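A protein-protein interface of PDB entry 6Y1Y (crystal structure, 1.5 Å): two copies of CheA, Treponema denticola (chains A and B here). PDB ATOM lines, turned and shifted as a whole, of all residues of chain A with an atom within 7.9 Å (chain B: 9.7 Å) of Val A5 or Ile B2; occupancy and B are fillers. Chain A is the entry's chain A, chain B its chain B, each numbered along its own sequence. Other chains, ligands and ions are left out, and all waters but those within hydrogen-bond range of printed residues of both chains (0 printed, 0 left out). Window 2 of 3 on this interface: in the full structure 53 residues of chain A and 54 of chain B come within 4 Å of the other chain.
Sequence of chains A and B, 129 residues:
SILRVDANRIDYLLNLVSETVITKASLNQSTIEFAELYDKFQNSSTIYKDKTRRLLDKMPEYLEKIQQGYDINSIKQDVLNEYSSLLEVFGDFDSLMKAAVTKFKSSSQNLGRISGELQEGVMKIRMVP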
ATOM      1  N   VAL A   5     -29.054 -21.980  16.083  1.00  0.00           N
ATOM      2  CA  VAL A   5     -28.120 -20.861  16.202  1.00  0.00           C
ATOM      3  C   VAL A   5     -28.402 -19.769  15.174  1.00  0.00           C
ATOM      4  O   VAL A   5     -28.942 -20.041  14.087  1.00  0.00           O
ATOM      5  CB  VAL A   5     -26.647 -21.317  16.079  1.00  0.00           C
ATOM      6  CG1 VAL A   5     -26.292 -22.312  17.190  1.00  0.00           C
ATOM      7  CG2 VAL A   5     -26.358 -21.910  14.707  1.00  0.00           C
ATOM      8  N   ASP A   6     -27.988 -18.542  15.511  1.00  0.00           N
ATOM      9  CA  ASP A   6     -28.148 -17.418  14.596  1.00  0.00           C
ATOM     10  C   ASP A   6     -27.242 -17.590  13.385  1.00  0.00           C
ATOM     11  O   ASP A   6     -26.053 -17.874  13.529  1.00  0.00           O
ATOM     12  CB  ASP A   6     -27.777 -16.101  15.276  1.00  0.00           C
ATOM     13  CG  ASP A   6     -28.194 -14.901  14.464  1.00  0.00           C
ATOM     14  OD1 ASP A   6     -29.182 -15.005  13.723  1.00  0.00           O
ATOM     15  OD2 ASP A   6     -27.454 -13.901  14.469  1.00  0.00           O
ATOM     16  N   ALA A   7     -27.803 -17.419  12.187  1.00  0.00           N
ATOM     17  CA  ALA A   7     -26.993 -17.538  10.977  1.00  0.00           C
ATOM     18  C   ALA A   7     -25.861 -16.512  10.967  1.00  0.00           C
ATOM     19  O   ALA A   7     -24.732 -16.823  10.569  1.00  0.00           O
ATOM     20  CB  ALA A   7     -27.868 -17.375   9.737  1.00  0.00           C
ATOM     21  N   ASN A   8     -26.147 -15.278  11.393  1.00  0.00           N
ATOM     22  CA  ASN A   8     -25.126 -14.237  11.406  1.00  0.00           C
ATOM     23  C   ASN A   8     -24.002 -14.556  12.385  1.00  0.00           C
ATOM     24  O   ASN A   8     -22.881 -14.066  12.207  1.00  0.00           O
ATOM     25  CB  ASN A   8     -25.763 -12.880  11.726  1.00  0.00           C
ATOM     26  CG  ASN A   8     -26.713 -12.414  10.638  1.00  0.00           C
ATOM     27  OD1 ASN A   8     -26.566 -12.767   9.465  1.00  0.00           O
ATOM     28  ND2 ASN A   8     -27.701 -11.617  11.025  1.00  0.00           N
ATOM     29  N   ARG A   9     -24.281 -15.327  13.446  1.00  0.00           N
ATOM     30  CA  ARG A   9     -23.208 -15.682  14.369  1.00  0.00           C
ATOM     31  C   ARG A   9     -22.226 -16.647  13.722  1.00  0.00           C
ATOM     32  O   ARG A   9     -21.014 -16.556  13.964  1.00  0.00           O
ATOM     33  CB  ARG A   9     -23.766 -16.340  15.634  1.00  0.00           C
ATOM     34  CG  ARG A   9     -24.640 -15.491  16.547  1.00  0.00           C
ATOM     35  CD  ARG A   9     -24.163 -14.062  16.717  1.00  0.00           C
ATOM     36  NE  ARG A   9     -25.216 -13.216  17.284  1.00  0.00           N
ATOM     37  CZ  ARG A   9     -25.601 -13.244  18.559  1.00  0.00           C
ATOM     38  NH1 ARG A   9     -25.021 -14.074  19.418  1.00  0.00           N
ATOM     39  NH2 ARG A   9     -26.567 -12.438  18.978  1.00  0.00           N
ATOM     40  N   ILE A  10     -22.721 -17.550  12.871  1.00  0.00           N
ATOM     41  CA  ILE A  10     -21.839 -18.479  12.174  1.00  0.00           C
ATOM     42  C   ILE A  10     -21.068 -17.761  11.076  1.00  0.00           C
ATOM     43  O   ILE A  10     -19.889 -18.050  10.837  1.00  0.00           O
ATOM     44  CB  ILE A  10     -22.641 -19.673  11.623  1.00  0.00           C
ATOM     45  CG1 ILE A  10     -23.387 -20.382  12.758  1.00  0.00           C
ATOM     46  CG2 ILE A  10     -21.711 -20.653  10.932  1.00  0.00           C
ATOM     47  CD1 ILE A  10     -22.475 -20.987  13.801  1.00  0.00           C
ATOM     48  N   LYS A 124     -19.794 -19.519  22.979  1.00  0.00           N
ATOM     49  CA  LYS A 124     -21.173 -19.092  23.142  1.00  0.00           C
ATOM     50  C   LYS A 124     -22.141 -19.965  22.372  1.00  0.00           C
ATOM     51  O   LYS A 124     -23.319 -20.015  22.730  1.00  0.00           O
ATOM     52  CB  LYS A 124     -21.304 -17.649  22.665  1.00  0.00           C
ATOM     53  CG  LYS A 124     -21.250 -16.634  23.791  1.00  0.00           C
ATOM     54  CD  LYS A 124     -22.570 -16.627  24.502  1.00  0.00           C
ATOM     55  CE  LYS A 124     -22.991 -15.224  24.890  1.00  0.00           C
ATOM     56  NZ  LYS A 124     -23.347 -14.355  23.724  1.00  0.00           N
ATOM     57  N   ILE A 125     -21.674 -20.636  21.320  1.00  0.00           N
ATOM     58  CA  ILE A 125     -22.483 -21.663  20.691  1.00  0.00           C
ATOM     59  C   ILE A 125     -22.468 -22.931  21.543  1.00  0.00           C
ATOM     60  O   ILE A 125     -23.449 -23.666  21.582  1.00  0.00           O
ATOM     61  CB  ILE A 125     -21.988 -21.919  19.260  1.00  0.00           C
ATOM     62  CG1 ILE A 125     -22.124 -20.647  18.420  1.00  0.00           C
ATOM     63  CG2 ILE A 125     -22.778 -23.037  18.620  1.00  0.00           C
ATOM     64  CD1 ILE A 125     -21.222 -20.638  17.207  1.00  0.00           C
ATOM     65  N   ARG A 126     -21.380 -23.201  22.263  1.00  0.00           N
ATOM     66  CA  ARG A 126     -21.337 -24.389  23.111  1.00  0.00           C
ATOM     67  C   ARG A 126     -22.317 -24.292  24.267  1.00  0.00           C
ATOM     68  O   ARG A 126     -22.610 -25.299  24.924  1.00  0.00           O
ATOM     69  CB  ARG A 126     -19.916 -24.579  23.647  1.00  0.00           C
ATOM     70  CG  ARG A 126     -19.713 -25.867  24.413  1.00  0.00           C
ATOM     71  CD  ARG A 126     -20.252 -27.054  23.638  1.00  0.00           C
ATOM     72  NE  ARG A 126     -20.263 -28.240  24.485  1.00  0.00           N
ATOM     73  CZ  ARG A 126     -21.181 -28.500  25.412  1.00  0.00           C
ATOM     74  NH1 ARG A 126     -22.196 -27.666  25.617  1.00  0.00           N
ATOM     75  NH2 ARG A 126     -21.081 -29.603  26.138  1.00  0.00           N
ATOM     76  N   VAL A 128     -25.528 -23.049  23.860  1.00  0.00           N
ATOM     77  CA  VAL A 128     -26.928 -23.051  23.441  1.00  0.00           C
ATOM     78  C   VAL A 128     -27.409 -24.463  23.763  1.00  0.00           C
ATOM     79  O   VAL A 128     -26.686 -25.428  23.465  1.00  0.00           O
ATOM     80  CB  VAL A 128     -27.108 -22.789  21.926  1.00  0.00           C
ATOM     81  CG1 VAL A 128     -27.063 -21.298  21.531  1.00  0.00           C
ATOM     82  CG2 VAL A 128     -26.490 -23.839  20.950  1.00  0.00           C
ATOM     83  N   PRO A 129     -28.619 -24.636  24.306  1.00  0.00           N
ATOM     84  CA  PRO A 129     -29.024 -26.022  24.564  1.00  0.00           C
ATOM     85  C   PRO A 129     -29.464 -26.771  23.309  1.00  0.00           C
ATOM     86  O   PRO A 129     -29.800 -26.150  22.301  1.00  0.00           O
ATOM     87  CB  PRO A 129     -30.195 -25.872  25.555  1.00  0.00           C
ATOM     88  CG  PRO A 129     -30.620 -24.451  25.435  1.00  0.00           C
ATOM     89  CD  PRO A 129     -29.422 -23.657  25.064  1.00  0.00           C
ATOM     90  N   ILE B   2     -31.268 -19.757  13.444  1.00  0.00           N
ATOM     91  CA  ILE B   2     -31.855 -20.190  12.183  1.00  0.00           C
ATOM     92  C   ILE B   2     -30.898 -21.108  11.426  1.00  0.00           C
ATOM     93  O   ILE B   2     -31.069 -21.349  10.230  1.00  0.00           O
ATOM     94  CB  ILE B   2     -32.255 -18.984  11.319  1.00  0.00           C
ATOM     95  CG1 ILE B   2     -31.154 -17.925  11.325  1.00  0.00           C
ATOM     96  CG2 ILE B   2     -33.569 -18.390  11.811  1.00  0.00           C
ATOM     97  CD1 ILE B   2     -31.416 -16.786  10.361  1.00  0.00           C
ATOM     98  N   LEU B   3     -29.885 -21.606  12.130  1.00  0.00           N
ATOM     99  CA  LEU B   3     -28.976 -22.620  11.619  1.00  0.00           C
ATOM    100  C   LEU B   3     -28.868 -23.716  12.670  1.00  0.00           C
ATOM    101  O   LEU B   3     -29.026 -23.461  13.866  1.00  0.00           O
ATOM    102  CB  LEU B   3     -27.575 -22.032  11.297  1.00  0.00           C
ATOM    103  CG  LEU B   3     -26.645 -22.723  10.288  1.00  0.00           C
ATOM    104  CD1 LEU B   3     -25.706 -21.724   9.619  1.00  0.00           C
ATOM    105  CD2 LEU B   3     -25.838 -23.827  10.941  1.00  0.00           C
ATOM    106  N   ARG B   4     -28.607 -24.938  12.219  1.00  0.00           N
ATOM    107  CA  ARG B   4     -28.410 -26.070  13.107  1.00  0.00           C
ATOM    108  C   ARG B   4     -26.956 -26.552  13.030  1.00  0.00           C
ATOM    109  O   ARG B   4     -26.430 -26.747  11.939  1.00  0.00           O
ATOM    110  N   VAL B   5     -26.349 -26.730  14.198  1.00  0.00           N
ATOM    111  CA  VAL B   5     -24.949 -27.139  14.262  1.00  0.00           C
ATOM    112  C   VAL B   5     -24.819 -28.404  15.098  1.00  0.00           C
ATOM    113  O   VAL B   5     -25.589 -28.641  16.033  1.00  0.00           O
ATOM    114  CB  VAL B   5     -24.045 -26.020  14.835  1.00  0.00           C
ATOM    115  CG1 VAL B   5     -24.114 -24.779  13.970  1.00  0.00           C
ATOM    116  CG2 VAL B   5     -24.432 -25.698  16.273  1.00  0.00           C
ATOM    117  N   ASP B   6     -23.824 -29.220  14.748  1.00  0.00           N
ATOM    118  CA  ASP B   6     -23.521 -30.431  15.500  1.00  0.00           C
ATOM    119  C   ASP B   6     -22.785 -30.074  16.787  1.00  0.00           C
ATOM    120  O   ASP B   6     -21.781 -29.353  16.755  1.00  0.00           O
ATOM    121  CB  ASP B   6     -22.672 -31.382  14.651  1.00  0.00           C
ATOM    122  CG  ASP B   6     -22.560 -32.767  15.257  1.00  0.00           C
ATOM    123  OD1 ASP B   6     -23.150 -33.710  14.692  1.00  0.00           O
ATOM    124  OD2 ASP B   6     -21.878 -32.916  16.293  1.00  0.00           O
ATOM    125  N   ALA B   7     -23.274 -30.591  17.915  1.00  0.00           N
ATOM    126  CA  ALA B   7     -22.635 -30.302  19.196  1.00  0.00           C
ATOM    127  C   ALA B   7     -21.209 -30.836  19.240  1.00  0.00           C
ATOM    128  O   ALA B   7     -20.295 -30.152  19.719  1.00  0.00           O
ATOM    129  CB  ALA B   7     -23.461 -30.882  20.344  1.00  0.00           C
ATOM    130  N   ILE B  10     -18.767 -28.731  17.341  1.00  0.00           N
ATOM    131  CA  ILE B  10     -18.454 -27.482  18.026  1.00  0.00           C
ATOM    132  C   ILE B  10     -17.384 -27.719  19.086  1.00  0.00           C
ATOM    133  O   ILE B  10     -16.477 -26.898  19.268  1.00  0.00           O
ATOM    134  CB  ILE B  10     -19.733 -26.878  18.635  1.00  0.00           C
ATOM    135  CG1 ILE B  10     -20.695 -26.433  17.528  1.00  0.00           C
ATOM    136  CG2 ILE B  10     -19.398 -25.728  19.581  1.00  0.00           C
ATOM    137  CD1 ILE B  10     -20.242 -25.204  16.778  1.00  0.00           C
ATOM    138  N   ILE B 125     -19.601 -27.127  10.010  1.00  0.00           N
ATOM    139  CA  ILE B 125     -20.624 -27.103  11.050  1.00  0.00           C
ATOM    140  C   ILE B 125     -21.955 -26.618  10.488  1.00  0.00           C
ATOM    141  O   ILE B 125     -23.011 -26.929  11.048  1.00  0.00           O
ATOM    142  CB  ILE B 125     -20.199 -26.250  12.264  1.00  0.00           C
ATOM    143  CG1 ILE B 125     -20.146 -24.763  11.901  1.00  0.00           C
ATOM    144  CG2 ILE B 125     -18.884 -26.750  12.843  1.00  0.00           C
ATOM    145  CD1 ILE B 125     -20.168 -23.839  13.099  1.00  0.00           C
ATOM    146  N   ARG B 126     -21.933 -25.834   9.408  1.00  0.00           N
ATOM    147  CA  ARG B 126     -23.156 -25.288   8.815  1.00  0.00           C
ATOM    148  C   ARG B 126     -24.011 -26.393   8.207  1.00  0.00           C
ATOM    149  O   ARG B 126     -23.607 -27.054   7.244  1.00  0.00           O
ATOM    150  CB  ARG B 126     -22.815 -24.243   7.761  1.00  0.00           C
ATOM    151  CG  ARG B 126     -22.158 -22.993   8.317  1.00  0.00           C
ATOM    152  CD  ARG B 126     -21.734 -22.086   7.187  1.00  0.00           C
ATOM    153  NE  ARG B 126     -20.842 -22.797   6.282  1.00  0.00           N
ATOM    154  CZ  ARG B 126     -20.442 -22.332   5.107  1.00  0.00           C
ATOM    155  NH1 ARG B 126     -20.847 -21.140   4.680  1.00  0.00           N
ATOM    156  NH2 ARG B 126     -19.632 -23.066   4.360  1.00  0.00           N
ATOM    157  N   MET B 127     -25.182 -26.616   8.786  1.00  0.00           N
ATOM    158  CA  MET B 127     -26.138 -27.579   8.269  1.00  0.00           C
ATOM    159  C   MET B 127     -27.434 -26.867   7.916  1.00  0.00           C
ATOM    160  O   MET B 127     -27.764 -25.822   8.482  1.00  0.00           O
ATOM    161  CB  MET B 127     -26.387 -28.708   9.276  1.00  0.00           C
ATOM    162  CG  MET B 127     -25.099 -29.406   9.687  1.00  0.00           C
ATOM    163  SD  MET B 127     -25.333 -30.798  10.804  1.00  0.00           S
ATOM    164  CE  MET B 127     -26.657 -30.208  11.852  1.00  0.00           C
ATOM    165  N   VAL B 128     -28.157 -27.434   6.959  1.00  0.00           N
ATOM    166  CA  VAL B 128     -29.534 -27.042   6.673  1.00  0.00           C
ATOM    167  C   VAL B 128     -30.442 -27.968   7.473  1.00  0.00           C
ATOM    168  O   VAL B 128     -29.968 -29.010   7.951  1.00  0.00           O
ATOM    169  CB  VAL B 128     -29.832 -27.093   5.169  1.00  0.00           C
ATOM    170  CG1 VAL B 128     -28.840 -26.214   4.440  1.00  0.00           C
ATOM    171  CG2 VAL B 128     -29.787 -28.528   4.668  1.00  0.00           C
ATOM    172  N   PRO B 129     -31.721 -27.614   7.711  1.00  0.00           N
ATOM    173  CA  PRO B 129     -32.441 -26.404   7.287  1.00  0.00           C
ATOM    174  C   PRO B 129     -32.069 -25.148   8.068  1.00  0.00           C
ATOM    175  O   PRO B 129     -32.404 -24.063   7.582  1.00  0.00           O
ATOM    176  CB  PRO B 129     -33.914 -26.774   7.518  1.00  0.00           C
ATOM    177  CG  PRO B 129     -33.886 -27.788   8.572  1.00  0.00           C
ATOM    178  CD  PRO B 129     -32.615 -28.570   8.390  1.00  0.00           C
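Hydrophobic or aromatic side chains of chain B that line the printed part of chain A: Ile B2, Leu B3, Val B5, Ile B10 and Ile B125.
Along chain A the printed residues that touch a printed residue of chain B span positions 5 to 125.
Among the printed residues, 8 pairs touch across the chains.
Among the printed residues, no Asp or Glu carboxylate lies within 4 Å of a Lys or Arg side-chain nitrogen of the other chain.
Val A5 touches just these residues of chain B: Ile B2 (2.4 Å), Leu B3 (2.7 Å) and Val B5 (3.7 Å).
Of the printed residues of chain B, Ala A7 touches Ile B2.
Asn A8 touches none of the printed residues of chain B.
Of the printed residues of chain B, Ile A125 touches Val B5 and Ile B10.
Printed residues of chain A within 4 Å of Ile B125: Ile A10.
Pro B129 touches none of the printed residues of chain A.
The nearest residue of chain B that does not touch Val A5 is Arg B4 (4.5 Å).
The nearest printed residue of chain A that does not touch Val B5 is Ile A10 (4.1 Å).
O of Leu B3 sits at hydrogen-bond distance from N of Val A5 (2.7 Å).
O of Val A5 sits at hydrogen-bond distance from N of Ile B2, at 2.4 Å.
Val B5 touches its own counterpart, Val A5.
Ile A10 touches Ile B125, and with the chains exchanged Ile A125 touches Ile B10.
Ile A10 touches Arg B126, but with the chains exchanged Arg A126 does not touch Ile B10 (4.2 Å).
Ile A125 touches Val B5, but with the chains exchanged Val A5 does not touch Ile B125 (6.7 Å).
8 positions are printed for both chains.
Of the 8 pairs that touch across the chains among the printed residues, 3 have their exchanged pair printed and touching as well.
Among the printed residues, merely in contact across the chains: Val A5 with Val B5 (3.7 Å), Ala A7 with Ile B2 (3.5 Å), Ile A10 with Ile B125 (3.7 Å), Ile A10 with Arg B126 (3.5 Å), Ile A125 with Val B5 (3.9 Å) and Ile A125 with Ile B10 (3.8 Å).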
